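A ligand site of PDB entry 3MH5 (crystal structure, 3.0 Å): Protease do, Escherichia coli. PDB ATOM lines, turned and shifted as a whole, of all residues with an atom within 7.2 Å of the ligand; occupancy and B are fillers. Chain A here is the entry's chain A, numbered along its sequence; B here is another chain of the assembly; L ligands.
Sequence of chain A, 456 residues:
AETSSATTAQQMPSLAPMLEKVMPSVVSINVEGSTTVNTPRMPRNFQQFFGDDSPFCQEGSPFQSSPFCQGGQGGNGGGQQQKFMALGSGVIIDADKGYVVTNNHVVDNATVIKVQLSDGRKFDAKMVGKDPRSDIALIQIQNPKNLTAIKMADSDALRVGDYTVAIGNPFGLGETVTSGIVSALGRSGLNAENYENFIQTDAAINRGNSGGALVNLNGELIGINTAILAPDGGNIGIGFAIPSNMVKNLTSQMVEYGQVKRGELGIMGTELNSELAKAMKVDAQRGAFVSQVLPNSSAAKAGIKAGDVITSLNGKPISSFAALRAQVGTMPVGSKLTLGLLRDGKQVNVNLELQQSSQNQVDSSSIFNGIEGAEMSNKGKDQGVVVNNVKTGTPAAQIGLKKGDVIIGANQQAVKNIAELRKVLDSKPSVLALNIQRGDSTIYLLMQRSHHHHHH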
ATOM      1  N   SER A  89     -15.298  20.507  33.644  1.00  0.00           N
ATOM      2  CA  SER A  89     -16.741  20.583  33.584  1.00  0.00           C
ATOM      3  C   SER A  89     -17.319  19.571  34.585  1.00  0.00           C
ATOM      4  O   SER A  89     -16.630  18.628  35.009  1.00  0.00           O
ATOM      5  CB  SER A  89     -17.199  20.255  32.159  1.00  0.00           C
ATOM      6  OG  SER A  89     -18.615  20.195  32.051  1.00  0.00           O
ATOM      7  N   VAL A 165     -24.974  13.659  22.926  1.00  0.00           N
ATOM      8  CA  VAL A 165     -24.456  15.021  22.925  1.00  0.00           C
ATOM      9  C   VAL A 165     -23.496  15.161  24.094  1.00  0.00           C
ATOM     10  O   VAL A 165     -23.791  14.727  25.208  1.00  0.00           O
ATOM     11  CB  VAL A 165     -25.578  16.067  23.065  1.00  0.00           C
ATOM     12  CG1 VAL A 165     -24.973  17.453  23.191  1.00  0.00           C
ATOM     13  CG2 VAL A 165     -26.474  16.020  21.847  1.00  0.00           C
ATOM     14  N   ALA A 166     -22.336  15.746  23.820  1.00  0.00           N
ATOM     15  CA  ALA A 166     -21.323  15.938  24.857  1.00  0.00           C
ATOM     16  C   ALA A 166     -21.205  17.415  25.206  1.00  0.00           C
ATOM     17  O   ALA A 166     -21.139  18.274  24.315  1.00  0.00           O
ATOM     18  CB  ALA A 166     -19.978  15.393  24.376  1.00  0.00           C
ATOM     19  N   ILE A 167     -21.195  17.699  26.503  1.00  0.00           N
ATOM     20  CA  ILE A 167     -21.103  19.070  27.007  1.00  0.00           C
ATOM     21  C   ILE A 167     -19.835  19.197  27.844  1.00  0.00           C
ATOM     22  O   ILE A 167     -19.572  18.342  28.670  1.00  0.00           O
ATOM     23  CB  ILE A 167     -22.326  19.393  27.885  1.00  0.00           C
ATOM     24  CG1 ILE A 167     -23.606  19.205  27.077  1.00  0.00           C
ATOM     25  CG2 ILE A 167     -22.217  20.818  28.420  1.00  0.00           C
ATOM     26  CD1 ILE A 167     -24.830  19.214  27.906  1.00  0.00           C
ATOM     27  N   GLY A 168     -19.070  20.264  27.632  1.00  0.00           N
ATOM     28  CA  GLY A 168     -17.835  20.437  28.387  1.00  0.00           C
ATOM     29  C   GLY A 168     -17.286  21.847  28.476  1.00  0.00           C
ATOM     30  O   GLY A 168     -17.899  22.796  28.001  1.00  0.00           O
ATOM     31  N   ASN A 169     -16.116  21.965  29.095  1.00  0.00           N
ATOM     32  CA  ASN A 169     -15.436  23.253  29.280  1.00  0.00           C
ATOM     33  C   ASN A 169     -13.987  23.116  28.817  1.00  0.00           C
ATOM     34  O   ASN A 169     -13.058  23.254  29.616  1.00  0.00           O
ATOM     35  CB  ASN A 169     -15.467  23.634  30.760  1.00  0.00           C
ATOM     36  CG  ASN A 169     -14.836  24.991  31.030  1.00  0.00           C
ATOM     37  OD1 ASN A 169     -14.560  25.337  32.174  1.00  0.00           O
ATOM     38  ND2 ASN A 169     -14.621  25.753  29.968  1.00  0.00           N
ATOM     39  N   PRO A 170     -13.775  22.881  27.516  1.00  0.00           N
ATOM     40  CA  PRO A 170     -12.462  22.717  26.905  1.00  0.00           C
ATOM     41  C   PRO A 170     -11.453  23.876  26.950  1.00  0.00           C
ATOM     42  O   PRO A 170     -10.257  23.635  26.797  1.00  0.00           O
ATOM     43  CB  PRO A 170     -12.798  22.316  25.475  1.00  0.00           C
ATOM     44  CG  PRO A 170     -14.026  23.113  25.215  1.00  0.00           C
ATOM     45  CD  PRO A 170     -14.832  22.896  26.480  1.00  0.00           C
ATOM     46  N   PHE A 171     -11.911  25.107  27.156  1.00  0.00           N
ATOM     47  CA  PHE A 171     -10.979  26.241  27.175  1.00  0.00           C
ATOM     48  C   PHE A 171     -11.204  27.193  28.337  1.00  0.00           C
ATOM     49  O   PHE A 171     -10.447  28.155  28.497  1.00  0.00           O
ATOM     50  CB  PHE A 171     -11.079  27.041  25.858  1.00  0.00           C
ATOM     51  CG  PHE A 171     -11.109  26.187  24.619  1.00  0.00           C
ATOM     52  CD1 PHE A 171     -12.192  26.259  23.737  1.00  0.00           C
ATOM     53  CD2 PHE A 171     -10.073  25.292  24.333  1.00  0.00           C
ATOM     54  CE1 PHE A 171     -12.242  25.461  22.588  1.00  0.00           C
ATOM     55  CE2 PHE A 171     -10.113  24.494  23.186  1.00  0.00           C
ATOM     56  CZ  PHE A 171     -11.198  24.582  22.316  1.00  0.00           C
ATOM     57  N   GLU A 175     -19.229  26.756  28.185  1.00  0.00           N
ATOM     58  CA  GLU A 175     -19.611  25.418  27.753  1.00  0.00           C
ATOM     59  C   GLU A 175     -19.519  25.220  26.254  1.00  0.00           C
ATOM     60  O   GLU A 175     -19.809  26.133  25.482  1.00  0.00           O
ATOM     61  CB  GLU A 175     -21.043  25.103  28.203  1.00  0.00           C
ATOM     62  CG  GLU A 175     -21.170  24.417  29.558  1.00  0.00           C
ATOM     63  CD  GLU A 175     -20.904  25.333  30.742  1.00  0.00           C
ATOM     64  OE1 GLU A 175     -19.717  25.514  31.096  1.00  0.00           O
ATOM     65  OE2 GLU A 175     -21.866  25.883  31.314  1.00  0.00           O
ATOM     66  N   THR A 176     -19.111  24.024  25.843  1.00  0.00           N
ATOM     67  CA  THR A 176     -19.006  23.652  24.427  1.00  0.00           C
ATOM     68  C   THR A 176     -19.814  22.381  24.205  1.00  0.00           C
ATOM     69  O   THR A 176     -19.657  21.402  24.914  1.00  0.00           O
ATOM     70  CB  THR A 176     -17.553  23.361  24.037  1.00  0.00           C
ATOM     71  OG1 THR A 176     -16.764  24.538  24.249  1.00  0.00           O
ATOM     72  CG2 THR A 176     -17.474  22.997  22.574  1.00  0.00           C
ATOM     73  N   VAL A 177     -20.694  22.416  23.214  1.00  0.00           N
ATOM     74  CA  VAL A 177     -21.537  21.259  22.935  1.00  0.00           C
ATOM     75  C   VAL A 177     -21.177  20.597  21.603  1.00  0.00           C
ATOM     76  O   VAL A 177     -20.968  21.283  20.609  1.00  0.00           O
ATOM     77  CB  VAL A 177     -23.019  21.671  22.925  1.00  0.00           C
ATOM     78  CG1 VAL A 177     -23.898  20.451  22.709  1.00  0.00           C
ATOM     79  CG2 VAL A 177     -23.376  22.343  24.227  1.00  0.00           C
ATOM     80  N   THR A 178     -21.091  19.274  21.592  1.00  0.00           N
ATOM     81  CA  THR A 178     -20.811  18.541  20.362  1.00  0.00           C
ATOM     82  C   THR A 178     -21.774  17.375  20.266  1.00  0.00           C
ATOM     83  O   THR A 178     -22.300  16.907  21.281  1.00  0.00           O
ATOM     84  CB  THR A 178     -19.363  18.015  20.320  1.00  0.00           C
ATOM     85  OG1 THR A 178     -19.097  17.251  21.492  1.00  0.00           O
ATOM     86  CG2 THR A 178     -18.394  19.167  20.268  1.00  0.00           C
ATOM     87  N   ALA A 203     -19.366  11.467  19.218  1.00  0.00           N
ATOM     88  CA  ALA A 203     -19.928  12.736  19.645  1.00  0.00           C
ATOM     89  C   ALA A 203     -18.962  13.539  20.498  1.00  0.00           C
ATOM     90  O   ALA A 203     -19.241  14.688  20.835  1.00  0.00           O
ATOM     91  CB  ALA A 203     -21.206  12.488  20.426  1.00  0.00           C
ATOM     92  N   ALA A 204     -17.836  12.927  20.850  1.00  0.00           N
ATOM     93  CA  ALA A 204     -16.823  13.601  21.661  1.00  0.00           C
ATOM     94  C   ALA A 204     -15.442  13.038  21.308  1.00  0.00           C
ATOM     95  O   ALA A 204     -15.166  11.867  21.569  1.00  0.00           O
ATOM     96  CB  ALA A 204     -17.122  13.394  23.159  1.00  0.00           C
ATOM     97  N   ILE A 205     -14.594  13.866  20.722  1.00  0.00           N
ATOM     98  CA  ILE A 205     -13.251  13.426  20.333  1.00  0.00           C
ATOM     99  C   ILE A 205     -12.453  13.026  21.568  1.00  0.00           C
ATOM    100  O   ILE A 205     -12.645  13.588  22.653  1.00  0.00           O
ATOM    101  CB  ILE A 205     -12.498  14.537  19.574  1.00  0.00           C
ATOM    102  CG1 ILE A 205     -13.394  15.129  18.488  1.00  0.00           C
ATOM    103  CG2 ILE A 205     -11.229  13.972  18.959  1.00  0.00           C
ATOM    104  CD1 ILE A 205     -13.908  14.116  17.471  1.00  0.00           C
ATOM    105  N   ASN A 206     -11.540  12.064  21.409  1.00  0.00           N
ATOM    106  CA  ASN A 206     -10.729  11.591  22.526  1.00  0.00           C
ATOM    107  C   ASN A 206      -9.731  12.669  22.962  1.00  0.00           C
ATOM    108  O   ASN A 206      -8.580  12.676  22.540  1.00  0.00           O
ATOM    109  CB  ASN A 206      -9.968  10.323  22.121  1.00  0.00           C
ATOM    110  CG  ASN A 206      -9.503   9.512  23.314  1.00  0.00           C
ATOM    111  OD1 ASN A 206      -8.753   8.552  23.165  1.00  0.00           O
ATOM    112  ND2 ASN A 206      -9.946   9.896  24.504  1.00  0.00           N
ATOM    113  N   ARG A 207     -10.195  13.572  23.825  1.00  0.00           N
ATOM    114  CA  ARG A 207      -9.355  14.661  24.328  1.00  0.00           C
ATOM    115  C   ARG A 207      -9.102  14.615  25.828  1.00  0.00           C
ATOM    116  O   ARG A 207     -10.018  14.339  26.623  1.00  0.00           O
ATOM    117  CB  ARG A 207      -9.986  16.015  23.981  1.00  0.00           C
ATOM    118  CG  ARG A 207      -9.502  16.628  22.682  1.00  0.00           C
ATOM    119  CD  ARG A 207      -9.839  15.755  21.499  1.00  0.00           C
ATOM    120  NE  ARG A 207      -9.006  16.094  20.341  1.00  0.00           N
ATOM    121  CZ  ARG A 207      -7.678  16.024  20.344  1.00  0.00           C
ATOM    122  NH1 ARG A 207      -7.025  15.633  21.432  1.00  0.00           N
ATOM    123  NH2 ARG A 207      -6.991  16.352  19.251  1.00  0.00           N
ATOM    124  N   GLY A 208      -7.858  14.879  26.212  1.00  0.00           N
ATOM    125  CA  GLY A 208      -7.515  14.884  27.620  1.00  0.00           C
ATOM    126  C   GLY A 208      -8.091  16.108  28.274  1.00  0.00           C
ATOM    127  O   GLY A 208      -7.919  16.333  29.468  1.00  0.00           O
ATOM    128  N   ASN A 209      -8.779  16.919  27.474  1.00  0.00           N
ATOM    129  CA  ASN A 209      -9.406  18.146  27.950  1.00  0.00           C
ATOM    130  C   ASN A 209     -10.922  17.987  27.845  1.00  0.00           C
ATOM    131  O   ASN A 209     -11.683  18.797  28.395  1.00  0.00           O
ATOM    132  CB  ASN A 209      -8.949  19.355  27.124  1.00  0.00           C
ATOM    133  CG  ASN A 209      -9.693  19.483  25.790  1.00  0.00           C
ATOM    134  OD1 ASN A 209      -9.613  18.598  24.940  1.00  0.00           O
ATOM    135  ND2 ASN A 209     -10.400  20.590  25.613  1.00  0.00           N
ATOM    136  N   SER A 210     -11.349  16.941  27.150  1.00  0.00           N
ATOM    137  CA  SER A 210     -12.777  16.674  26.984  1.00  0.00           C
ATOM    138  C   SER A 210     -13.302  15.636  27.958  1.00  0.00           C
ATOM    139  O   SER A 210     -13.015  14.439  27.836  1.00  0.00           O
ATOM    140  CB  SER A 210     -13.103  16.230  25.560  1.00  0.00           C
ATOM    141  OG  SER A 210     -13.472  17.339  24.752  1.00  0.00           O
ATOM    142  N   GLY A 211     -14.054  16.119  28.928  1.00  0.00           N
ATOM    143  CA  GLY A 211     -14.683  15.268  29.908  1.00  0.00           C
ATOM    144  C   GLY A 211     -16.138  15.687  29.842  1.00  0.00           C
ATOM    145  O   GLY A 211     -16.748  15.672  28.766  1.00  0.00           O
ATOM    146  N   GLY A 212     -16.694  16.090  30.960  1.00  0.00           N
ATOM    147  CA  GLY A 212     -18.076  16.523  30.950  1.00  0.00           C
ATOM    148  C   GLY A 212     -19.108  15.434  30.742  1.00  0.00           C
ATOM    149  O   GLY A 212     -18.811  14.229  30.716  1.00  0.00           O
ATOM    150  N   ALA A 213     -20.343  15.889  30.587  1.00  0.00           N
ATOM    151  CA  ALA A 213     -21.502  15.027  30.412  1.00  0.00           C
ATOM    152  C   ALA A 213     -21.721  14.425  29.031  1.00  0.00           C
ATOM    153  O   ALA A 213     -21.346  14.985  28.007  1.00  0.00           O
ATOM    154  CB  ALA A 213     -22.742  15.805  30.828  1.00  0.00           C
ATOM    155  N   LEU A 214     -22.342  13.256  29.029  1.00  0.00           N
ATOM    156  CA  LEU A 214     -22.706  12.576  27.801  1.00  0.00           C
ATOM    157  C   LEU A 214     -24.240  12.462  27.953  1.00  0.00           C
ATOM    158  O   LEU A 214     -24.742  11.786  28.864  1.00  0.00           O
ATOM    159  CB  LEU A 214     -21.999  11.212  27.719  1.00  0.00           C
ATOM    160  CG  LEU A 214     -21.583  10.761  26.313  1.00  0.00           C
ATOM    161  CD1 LEU A 214     -22.672   9.945  25.664  1.00  0.00           C
ATOM    162  CD2 LEU A 214     -21.254  11.988  25.462  1.00  0.00           C
ATOM    163  N   ASN A 225     -17.936  11.713  30.120  1.00  0.00           N
ATOM    164  CA  ASN A 225     -16.812  11.579  29.212  1.00  0.00           C
ATOM    165  C   ASN A 225     -15.453  11.650  29.952  1.00  0.00           C
ATOM    166  O   ASN A 225     -15.283  12.407  30.918  1.00  0.00           O
ATOM    167  CB  ASN A 225     -16.910  12.657  28.143  1.00  0.00           C
ATOM    168  CG  ASN A 225     -18.041  12.395  27.167  1.00  0.00           C
ATOM    169  OD1 ASN A 225     -18.810  13.294  26.841  1.00  0.00           O
ATOM    170  ND2 ASN A 225     -18.126  11.162  26.679  1.00  0.00           N
ATOM    171  N   GLY A 239     -14.372   8.794  21.324  1.00  0.00           N
ATOM    172  CA  GLY A 239     -14.347   8.983  22.765  1.00  0.00           C
ATOM    173  C   GLY A 239     -14.919   7.865  23.623  1.00  0.00           C
ATOM    174  O   GLY A 239     -15.736   7.060  23.161  1.00  0.00           O
ATOM    175  N   SER B 183     -21.106  24.727  18.445  1.00  0.00           N
ATOM    176  CA  SER B 183     -20.574  24.292  19.728  1.00  0.00           C
ATOM    177  C   SER B 183     -20.617  25.397  20.773  1.00  0.00           C
ATOM    178  O   SER B 183     -21.182  25.217  21.851  1.00  0.00           O
ATOM    179  CB  SER B 183     -19.133  23.798  19.559  1.00  0.00           C
ATOM    180  OG  SER B 183     -19.097  22.700  18.670  1.00  0.00           O
ATOM    181  N   GLN B 200     -18.011  28.909  17.107  1.00  0.00           N
ATOM    182  CA  GLN B 200     -17.300  27.642  17.263  1.00  0.00           C
ATOM    183  C   GLN B 200     -18.269  26.486  16.935  1.00  0.00           C
ATOM    184  O   GLN B 200     -19.414  26.463  17.397  1.00  0.00           O
ATOM    185  CB  GLN B 200     -16.809  27.551  18.701  1.00  0.00           C
ATOM    186  CG  GLN B 200     -15.873  26.425  18.999  1.00  0.00           C
ATOM    187  CD  GLN B 200     -15.193  26.626  20.337  1.00  0.00           C
ATOM    188  OE1 GLN B 200     -15.837  26.929  21.344  1.00  0.00           O
ATOM    189  NE2 GLN B 200     -13.875  26.458  20.352  1.00  0.00           N
ATOM    190  N   ASP B 202     -18.447  21.994  15.572  1.00  0.00           N
ATOM    191  CA  ASP B 202     -17.809  20.707  15.279  1.00  0.00           C
ATOM    192  C   ASP B 202     -18.082  20.316  13.825  1.00  0.00           C
ATOM    193  O   ASP B 202     -17.618  19.276  13.348  1.00  0.00           O
ATOM    194  CB  ASP B 202     -18.332  19.625  16.245  1.00  0.00           C
ATOM    195  CG  ASP B 202     -19.832  19.367  16.091  1.00  0.00           C
ATOM    196  OD1 ASP B 202     -20.568  20.277  15.638  1.00  0.00           O
ATOM    197  OD2 ASP B 202     -20.289  18.260  16.429  1.00  0.00           O
ATOM    198  N   ILE B 238     -12.009  21.381  17.038  1.00  0.00           N
ATOM    199  CA  ILE B 238     -13.232  22.122  16.736  1.00  0.00           C
ATOM    200  C   ILE B 238     -12.881  23.340  15.868  1.00  0.00           C
ATOM    201  O   ILE B 238     -11.710  23.731  15.788  1.00  0.00           O
ATOM    202  CB  ILE B 238     -13.931  22.562  18.056  1.00  0.00           C
ATOM    203  CG1 ILE B 238     -15.439  22.612  17.857  1.00  0.00           C
ATOM    204  CG2 ILE B 238     -13.411  23.932  18.513  1.00  0.00           C
ATOM    205  CD1 ILE B 238     -16.202  22.763  19.153  1.00  0.00           C
ATOM    206  N   GLY B 239     -13.887  23.941  15.242  1.00  0.00           N
ATOM    207  CA  GLY B 239     -13.627  25.091  14.389  1.00  0.00           C
ATOM    208  C   GLY B 239     -14.182  26.435  14.834  1.00  0.00           C
ATOM    209  O   GLY B 239     -15.141  26.506  15.611  1.00  0.00           O
HETATM  210  C1  LIG L   1     -16.459  18.125  24.864  1.00  0.00           C
HETATM  211  C2  LIG L   1     -17.016  17.166  25.945  1.00  0.00           C
HETATM  212  C3  LIG L   1     -17.509  19.174  24.321  1.00  0.00           C
HETATM  213  C4  LIG L   1     -13.580  19.580  22.526  1.00  0.00           C
HETATM  214  C5  LIG L   1     -14.113  20.389  21.311  1.00  0.00           C
HETATM  215  C6  LIG L   1     -12.047  19.609  22.572  1.00  0.00           C
HETATM  216  P1  LIG L   1     -14.415  17.155  23.527  1.00  0.00           P
HETATM  217  O1  LIG L   1     -15.974  17.300  23.798  1.00  0.00           O
HETATM  218  O2  LIG L   1     -14.013  18.226  22.377  1.00  0.00           O
HETATM  219  O3  LIG L   1     -14.109  15.744  23.057  1.00  0.00           O
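The backbone carbonyl oxygen of Gly 168 lies within hydrogen-bond range of the backbone NH of Thr 176 (2.8 Å). The backbone carbonyl oxygen (O) of Ala 204 lies within hydrogen-bond range of the backbone NH (N) of Gly 239 of chain A (3.2 Å). The side-chain amide nitrogen (ND2) of Asn 209 sits close to the backbone carbonyl oxygen (O) of Pro 170 (3.3 Å). The backbone NH (N) of Ala 166 sits at hydrogen-bond distance from the backbone carbonyl oxygen (O) of Thr 178, at 2.8 Å. The side-chain hydroxyl of Thr 178 lies within hydrogen-bond range of the backbone carbonyl oxygen of Ala 203, at 2.6 Å. O of Ala 213 is in hydrogen-bond range of N of Ile 167, 3.1 Å away.
Ala 166 touches the ligand. O of Ile 167 touches C2 of the ligand, at 3.9 Å. N of Gly 168 touches C3 of the ligand, at 3.8 Å. O of Thr 176 touches C3 of the ligand, 3.2 Å away. Thr 178 touches the ligand (OG1 to C3, 3.8 Å). C of Ala 204 touches O3 of the ligand, at 3.5 Å. Arg 207 touches the ligand (CG to C6, 3.9 Å). OD1 of Asn 209 touches C6 of the ligand, at 3.5 Å. O of Gly 211 touches C2 of the ligand, 3.2 Å away. Ile 238 of chain B touches the ligand (CD1 to C5, 3.8 Å). Hydrophobic or aromatic side chains that line the ligand: Ala 166, Ala 204 and Ile 238 of chain B. 12 residues have an atom within 4 Å of the ligand: Ala 166, Ile 167, Gly 168, Thr 176, Thr 178, Ala 204, Ile 205, Arg 207, Asn 209, Ser 210, Gly 211 and Ile 238 of chain B.
The side-chain hydroxyl of Ser 210 is covalently linked to a phosphorus (P1) of the ligand (1.6 Å). N of Ile 205 is in hydrogen-bond range of O3 of the ligand. The backbone carbonyl oxygen of Ile 205 sits close to an oxygen (O3) of the ligand.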
